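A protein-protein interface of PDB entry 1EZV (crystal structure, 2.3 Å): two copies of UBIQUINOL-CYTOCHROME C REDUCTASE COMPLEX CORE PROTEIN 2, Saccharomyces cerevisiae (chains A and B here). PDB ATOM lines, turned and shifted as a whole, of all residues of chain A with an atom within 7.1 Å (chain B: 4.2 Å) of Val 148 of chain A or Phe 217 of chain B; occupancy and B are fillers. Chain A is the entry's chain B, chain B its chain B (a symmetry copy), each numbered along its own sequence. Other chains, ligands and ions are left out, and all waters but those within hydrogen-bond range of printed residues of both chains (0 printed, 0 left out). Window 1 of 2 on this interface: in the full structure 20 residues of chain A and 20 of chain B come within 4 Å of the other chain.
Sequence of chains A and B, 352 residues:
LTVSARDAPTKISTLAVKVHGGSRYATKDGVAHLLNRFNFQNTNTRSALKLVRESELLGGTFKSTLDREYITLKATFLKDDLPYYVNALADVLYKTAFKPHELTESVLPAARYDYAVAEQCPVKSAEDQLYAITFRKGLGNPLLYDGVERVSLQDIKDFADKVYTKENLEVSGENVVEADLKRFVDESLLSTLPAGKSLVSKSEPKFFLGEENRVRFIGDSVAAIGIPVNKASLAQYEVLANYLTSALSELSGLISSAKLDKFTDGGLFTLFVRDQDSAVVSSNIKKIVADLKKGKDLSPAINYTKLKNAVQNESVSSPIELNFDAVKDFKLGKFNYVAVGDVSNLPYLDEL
The guanidinium group (NH1) of Arg 216 of chain B is in salt-bridge range of the side-chain carboxylate (OD2) of Asp 29 of chain A (2.8 Å). The guanidinium group of Arg 216 of chain B is in salt-bridge range of the side-chain carboxylate of Asp 146 of chain A, at 2.8 Å.
Hydrophobic or aromatic side chains of chain A within 4 Å of the printed part of chain B: Pro 142 and Val 148. Among the printed residues, Asp or Glu carboxylates within 4 Å of a Lys or Arg side-chain nitrogen of the other chain: Asp 29 of chain A with Arg 216 of chain B (2.8 Å) and Asp 146 of chain A with Arg 216 of chain B (2.8 Å).
No position is printed for both chains. Of the 7 pairs that touch across the chains among the printed residues, none has its exchanged pair printed and touching as well.
The side-chain carboxylate of Glu 149 of chain A sits at hydrogen-bond distance from the backbone NH of Asp 29 of chain A, at 3.0 Å. N of Val 148 of chain A sits close to OD1 of Asp 146 of chain A. The backbone carbonyl oxygen (O) of Gly 341 of chain B lies within hydrogen-bond range of the backbone NH (N) of Phe 217 of chain B.
Of the printed residues of chain B, Asp 146 of chain A touches Arg 216 and Ile 218. Printed residues of chain B within 4 Å of Gly 147 of chain A: Ile 218 (3.98 Å). Of chain B, only Arg 216 (3.1 Å) and Phe 217 (3.7 Å) come within 4 Å of Val 148 of chain A. Arg 150 of chain A touches none of the printed residues of chain B. Phe 217 of chain B touches just one residue of chain A: Val 148. The nearest residue of chain A that does not touch Phe 217 of chain B is Gly 147 of chain A (6.0 Å). The nearest printed residue of chain A that does not touch Arg 216 of chain B is Gly 147 of chain A (6.1 Å).
Among the printed residues, pairs that only touch across the chains: Pro 142 of chain A with Arg 216 of chain B (3.1 Å), Asp 146 of chain A with Ile 218 of chain B (3.3 Å), Gly 147 of chain A with Ile 218 of chain B (3.98 Å), Val 148 of chain A with Arg 216 of chain B (3.1 Å) and Val 148 of chain A with Phe 217 of chain B (3.7 Å).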
ATOM      1  N   ASP A  29      23.858 -30.062  29.190  1.00  0.00           N
ATOM      2  CA  ASP A  29      23.940 -30.215  27.738  1.00  0.00           C
ATOM      3  C   ASP A  29      24.955 -29.285  27.080  1.00  0.00           C
ATOM      4  O   ASP A  29      24.892 -28.064  27.237  1.00  0.00           O
ATOM      5  CB  ASP A  29      22.561 -30.006  27.106  1.00  0.00           C
ATOM      6  CG  ASP A  29      21.650 -31.209  27.280  1.00  0.00           C
ATOM      7  OD1 ASP A  29      21.706 -31.859  28.344  1.00  0.00           O
ATOM      8  OD2 ASP A  29      20.875 -31.508  26.350  1.00  0.00           O
ATOM      9  N   ARG A 112      28.854 -21.239  18.985  1.00  0.00           N
ATOM     10  CA  ARG A 112      27.651 -20.906  18.217  1.00  0.00           C
ATOM     11  C   ARG A 112      27.863 -21.188  16.728  1.00  0.00           C
ATOM     12  O   ARG A 112      26.954 -21.655  16.041  1.00  0.00           O
ATOM     13  CB  ARG A 112      27.288 -19.427  18.411  1.00  0.00           C
ATOM     14  CG  ARG A 112      25.848 -19.170  18.821  1.00  0.00           C
ATOM     15  CD  ARG A 112      25.676 -19.212  20.338  1.00  0.00           C
ATOM     16  NE  ARG A 112      24.397 -19.816  20.725  1.00  0.00           N
ATOM     17  CZ  ARG A 112      23.834 -19.708  21.928  1.00  0.00           C
ATOM     18  NH1 ARG A 112      22.701 -20.353  22.187  1.00  0.00           N
ATOM     19  NH2 ARG A 112      24.382 -18.939  22.864  1.00  0.00           N
ATOM     20  N   PRO A 142      23.504 -34.840  23.584  1.00  0.00           N
ATOM     21  CA  PRO A 142      23.922 -33.856  22.581  1.00  0.00           C
ATOM     22  C   PRO A 142      25.428 -33.626  22.565  1.00  0.00           C
ATOM     23  O   PRO A 142      26.051 -33.434  23.612  1.00  0.00           O
ATOM     24  CB  PRO A 142      23.170 -32.596  22.993  1.00  0.00           C
ATOM     25  CG  PRO A 142      21.954 -33.112  23.657  1.00  0.00           C
ATOM     26  CD  PRO A 142      22.410 -34.317  24.420  1.00  0.00           C
ATOM     27  N   LEU A 144      26.967 -31.049  20.803  1.00  0.00           N
ATOM     28  CA  LEU A 144      27.264 -29.620  20.824  1.00  0.00           C
ATOM     29  C   LEU A 144      26.254 -28.806  21.638  1.00  0.00           C
ATOM     30  O   LEU A 144      25.103 -29.223  21.839  1.00  0.00           O
ATOM     31  CB  LEU A 144      27.343 -29.079  19.390  1.00  0.00           C
ATOM     32  CG  LEU A 144      28.250 -29.836  18.408  1.00  0.00           C
ATOM     33  CD1 LEU A 144      28.139 -29.223  17.027  1.00  0.00           C
ATOM     34  CD2 LEU A 144      29.695 -29.811  18.876  1.00  0.00           C
ATOM     35  N   TYR A 145      26.712 -27.657  22.132  1.00  0.00           N
ATOM     36  CA  TYR A 145      25.886 -26.745  22.918  1.00  0.00           C
ATOM     37  C   TYR A 145      24.893 -25.985  22.034  1.00  0.00           C
ATOM     38  O   TYR A 145      25.251 -25.519  20.953  1.00  0.00           O
ATOM     39  CB  TYR A 145      26.790 -25.759  23.664  1.00  0.00           C
ATOM     40  CG  TYR A 145      26.056 -24.692  24.445  1.00  0.00           C
ATOM     41  CD1 TYR A 145      26.052 -23.363  24.013  1.00  0.00           C
ATOM     42  CD2 TYR A 145      25.384 -25.002  25.627  1.00  0.00           C
ATOM     43  CE1 TYR A 145      25.394 -22.366  24.739  1.00  0.00           C
ATOM     44  CE2 TYR A 145      24.730 -24.011  26.362  1.00  0.00           C
ATOM     45  CZ  TYR A 145      24.737 -22.697  25.909  1.00  0.00           C
ATOM     46  OH  TYR A 145      24.067 -21.723  26.614  1.00  0.00           O
ATOM     47  N   ASP A 146      23.641 -25.899  22.478  1.00  0.00           N
ATOM     48  CA  ASP A 146      22.624 -25.123  21.772  1.00  0.00           C
ATOM     49  C   ASP A 146      21.709 -24.316  22.697  1.00  0.00           C
ATOM     50  O   ASP A 146      20.690 -23.773  22.263  1.00  0.00           O
ATOM     51  CB  ASP A 146      21.788 -26.025  20.844  1.00  0.00           C
ATOM     52  CG  ASP A 146      21.044 -27.140  21.588  1.00  0.00           C
ATOM     53  OD1 ASP A 146      20.294 -26.852  22.545  1.00  0.00           O
ATOM     54  OD2 ASP A 146      21.118 -28.299  21.124  1.00  0.00           O
ATOM     55  N   GLY A 147      22.028 -24.325  23.986  1.00  0.00           N
ATOM     56  CA  GLY A 147      21.368 -23.438  24.925  1.00  0.00           C
ATOM     57  C   GLY A 147      19.977 -23.822  25.389  1.00  0.00           C
ATOM     58  O   GLY A 147      19.285 -22.985  25.965  1.00  0.00           O
ATOM     59  N   VAL A 148      19.592 -25.090  25.238  1.00  0.00           N
ATOM     60  CA  VAL A 148      18.277 -25.539  25.713  1.00  0.00           C
ATOM     61  C   VAL A 148      18.146 -25.554  27.235  1.00  0.00           C
ATOM     62  O   VAL A 148      17.064 -25.298  27.770  1.00  0.00           O
ATOM     63  CB  VAL A 148      17.904 -26.935  25.179  1.00  0.00           C
ATOM     64  CG1 VAL A 148      17.373 -26.816  23.759  1.00  0.00           C
ATOM     65  CG2 VAL A 148      19.105 -27.869  25.249  1.00  0.00           C
ATOM     66  N   GLU A 149      19.231 -25.893  27.927  1.00  0.00           N
ATOM     67  CA  GLU A 149      19.313 -25.623  29.360  1.00  0.00           C
ATOM     68  C   GLU A 149      20.532 -24.765  29.690  1.00  0.00           C
ATOM     69  O   GLU A 149      21.555 -24.830  28.997  1.00  0.00           O
ATOM     70  CB  GLU A 149      19.321 -26.929  30.180  1.00  0.00           C
ATOM     71  CG  GLU A 149      20.486 -27.890  29.926  1.00  0.00           C
ATOM     72  CD  GLU A 149      20.525 -29.063  30.917  1.00  0.00           C
ATOM     73  OE1 GLU A 149      21.166 -30.089  30.601  1.00  0.00           O
ATOM     74  OE2 GLU A 149      19.941 -28.955  32.022  1.00  0.00           O
ATOM     75  N   ARG A 150      20.375 -23.899  30.692  1.00  0.00           N
ATOM     76  CA  ARG A 150      21.409 -22.941  31.085  1.00  0.00           C
ATOM     77  C   ARG A 150      22.730 -23.636  31.396  1.00  0.00           C
ATOM     78  O   ARG A 150      22.750 -24.695  32.018  1.00  0.00           O
ATOM     79  CB  ARG A 150      20.975 -22.144  32.324  1.00  0.00           C
ATOM     80  CG  ARG A 150      19.478 -22.057  32.553  1.00  0.00           C
ATOM     81  CD  ARG A 150      18.875 -20.838  31.878  1.00  0.00           C
ATOM     82  NE  ARG A 150      17.442 -20.724  32.150  1.00  0.00           N
ATOM     83  CZ  ARG A 150      16.626 -19.860  31.550  1.00  0.00           C
ATOM     84  NH1 ARG A 150      15.337 -19.838  31.864  1.00  0.00           N
ATOM     85  NH2 ARG A 150      17.098 -19.016  30.641  1.00  0.00           N
ATOM     86  N   GLU B 119       5.850 -20.853  15.528  1.00  0.00           N
ATOM     87  CA  GLU B 119       7.149 -21.476  15.764  1.00  0.00           C
ATOM     88  C   GLU B 119       7.689 -21.171  17.162  1.00  0.00           C
ATOM     89  O   GLU B 119       8.635 -21.807  17.621  1.00  0.00           O
ATOM     90  CB  GLU B 119       8.147 -20.997  14.708  1.00  0.00           C
ATOM     91  CG  GLU B 119       9.480 -21.742  14.687  1.00  0.00           C
ATOM     92  CD  GLU B 119      10.507 -21.096  13.763  1.00  0.00           C
ATOM     93  OE1 GLU B 119      11.441 -21.805  13.332  1.00  0.00           O
ATOM     94  OE2 GLU B 119      10.396 -19.877  13.488  1.00  0.00           O
ATOM     95  N   GLN B 120       7.054 -20.229  17.851  1.00  0.00           N
ATOM     96  CA  GLN B 120       7.562 -19.749  19.131  1.00  0.00           C
ATOM     97  C   GLN B 120       6.636 -20.030  20.316  1.00  0.00           C
ATOM     98  O   GLN B 120       6.950 -19.667  21.450  1.00  0.00           O
ATOM     99  CB  GLN B 120       7.857 -18.249  19.037  1.00  0.00           C
ATOM    100  CG  GLN B 120       9.151 -17.920  18.296  1.00  0.00           C
ATOM    101  CD  GLN B 120       9.010 -16.722  17.369  1.00  0.00           C
ATOM    102  OE1 GLN B 120       9.385 -16.785  16.194  1.00  0.00           O
ATOM    103  NE2 GLN B 120       8.453 -15.628  17.888  1.00  0.00           N
ATOM    104  N   PRO B 122       5.221 -23.173  22.363  1.00  0.00           N
ATOM    105  CA  PRO B 122       5.707 -24.555  22.405  1.00  0.00           C
ATOM    106  C   PRO B 122       4.600 -25.591  22.612  1.00  0.00           C
ATOM    107  O   PRO B 122       4.826 -26.784  22.427  1.00  0.00           O
ATOM    108  CB  PRO B 122       6.706 -24.541  23.560  1.00  0.00           C
ATOM    109  CG  PRO B 122       6.167 -23.512  24.488  1.00  0.00           C
ATOM    110  CD  PRO B 122       5.485 -22.466  23.631  1.00  0.00           C
ATOM    111  N   VAL B 215      11.159 -32.941  21.076  1.00  0.00           N
ATOM    112  CA  VAL B 215      11.726 -31.788  20.375  1.00  0.00           C
ATOM    113  C   VAL B 215      12.426 -30.826  21.332  1.00  0.00           C
ATOM    114  O   VAL B 215      11.817 -30.311  22.276  1.00  0.00           O
ATOM    115  CB  VAL B 215      10.648 -30.995  19.598  1.00  0.00           C
ATOM    116  CG1 VAL B 215      11.314 -30.039  18.623  1.00  0.00           C
ATOM    117  CG2 VAL B 215       9.723 -31.944  18.857  1.00  0.00           C
ATOM    118  N   ARG B 216      13.701 -30.568  21.056  1.00  0.00           N
ATOM    119  CA  ARG B 216      14.490 -29.602  21.815  1.00  0.00           C
ATOM    120  C   ARG B 216      14.041 -28.181  21.486  1.00  0.00           C
ATOM    121  O   ARG B 216      13.794 -27.851  20.325  1.00  0.00           O
ATOM    122  CB  ARG B 216      15.974 -29.764  21.490  1.00  0.00           C
ATOM    123  CG  ARG B 216      16.339 -31.119  20.912  1.00  0.00           C
ATOM    124  CD  ARG B 216      17.835 -31.253  20.693  1.00  0.00           C
ATOM    125  NE  ARG B 216      18.534 -31.608  21.925  1.00  0.00           N
ATOM    126  CZ  ARG B 216      19.030 -30.726  22.786  1.00  0.00           C
ATOM    127  NH1 ARG B 216      19.616 -31.137  23.900  1.00  0.00           N
ATOM    128  NH2 ARG B 216      18.944 -29.430  22.531  1.00  0.00           N
ATOM    129  N   PHE B 217      13.925 -27.349  22.516  1.00  0.00           N
ATOM    130  CA  PHE B 217      13.336 -26.024  22.370  1.00  0.00           C
ATOM    131  C   PHE B 217      13.891 -25.070  23.418  1.00  0.00           C
ATOM    132  O   PHE B 217      13.932 -25.394  24.606  1.00  0.00           O
ATOM    133  CB  PHE B 217      11.812 -26.117  22.509  1.00  0.00           C
ATOM    134  CG  PHE B 217      11.092 -24.821  22.247  1.00  0.00           C
ATOM    135  CD1 PHE B 217      10.778 -24.436  20.947  1.00  0.00           C
ATOM    136  CD2 PHE B 217      10.669 -24.017  23.303  1.00  0.00           C
ATOM    137  CE1 PHE B 217      10.048 -23.272  20.702  1.00  0.00           C
ATOM    138  CE2 PHE B 217       9.941 -22.852  23.068  1.00  0.00           C
ATOM    139  CZ  PHE B 217       9.629 -22.480  21.765  1.00  0.00           C
ATOM    140  N   ILE B 218      14.314 -23.892  22.967  1.00  0.00           N
ATOM    141  CA  ILE B 218      14.734 -22.829  23.872  1.00  0.00           C
ATOM    142  C   ILE B 218      13.520 -22.004  24.310  1.00  0.00           C
ATOM    143  O   ILE B 218      12.879 -21.333  23.495  1.00  0.00           O
ATOM    144  CB  ILE B 218      15.780 -21.913  23.201  1.00  0.00           C
ATOM    145  CG1 ILE B 218      16.975 -22.747  22.733  1.00  0.00           C
ATOM    146  CG2 ILE B 218      16.244 -20.846  24.175  1.00  0.00           C
ATOM    147  CD1 ILE B 218      17.978 -21.982  21.898  1.00  0.00           C
ATOM    148  N   GLY B 219      13.161 -22.133  25.584  1.00  0.00           N
ATOM    149  CA  GLY B 219      11.989 -21.452  26.110  1.00  0.00           C
ATOM    150  C   GLY B 219      11.347 -22.250  27.230  1.00  0.00           C
ATOM    151  O   GLY B 219      12.042 -22.925  27.989  1.00  0.00           O
ATOM    152  N   ASP B 220      10.020 -22.192  27.321  1.00  0.00           N
ATOM    153  CA  ASP B 220       9.271 -23.005  28.280  1.00  0.00           C
ATOM    154  C   ASP B 220       9.277 -24.486  27.896  1.00  0.00           C
ATOM    155  O   ASP B 220       9.325 -24.831  26.714  1.00  0.00           O
ATOM    156  CB  ASP B 220       7.823 -22.515  28.376  1.00  0.00           C
ATOM    157  CG  ASP B 220       7.673 -21.279  29.250  1.00  0.00           C
ATOM    158  OD1 ASP B 220       6.518 -20.864  29.478  1.00  0.00           O
ATOM    159  OD2 ASP B 220       8.696 -20.717  29.704  1.00  0.00           O
ATOM    160  N   VAL B 340       8.588 -31.395  24.777  1.00  0.00           N
ATOM    161  CA  VAL B 340       9.116 -30.218  24.096  1.00  0.00           C
ATOM    162  C   VAL B 340       9.805 -29.311  25.111  1.00  0.00           C
ATOM    163  O   VAL B 340       9.196 -28.897  26.102  1.00  0.00           O
ATOM    164  CB  VAL B 340       7.987 -29.422  23.395  1.00  0.00           C
ATOM    165  CG1 VAL B 340       8.556 -28.183  22.714  1.00  0.00           C
ATOM    166  CG2 VAL B 340       7.273 -30.301  22.379  1.00  0.00           C
ATOM    167  N   GLY B 341      11.094 -29.068  24.895  1.00  0.00           N
ATOM    168  CA  GLY B 341      11.810 -28.099  25.705  1.00  0.00           C
ATOM    169  C   GLY B 341      13.137 -28.612  26.218  1.00  0.00           C
ATOM    170  O   GLY B 341      13.987 -29.050  25.440  1.00  0.00           O
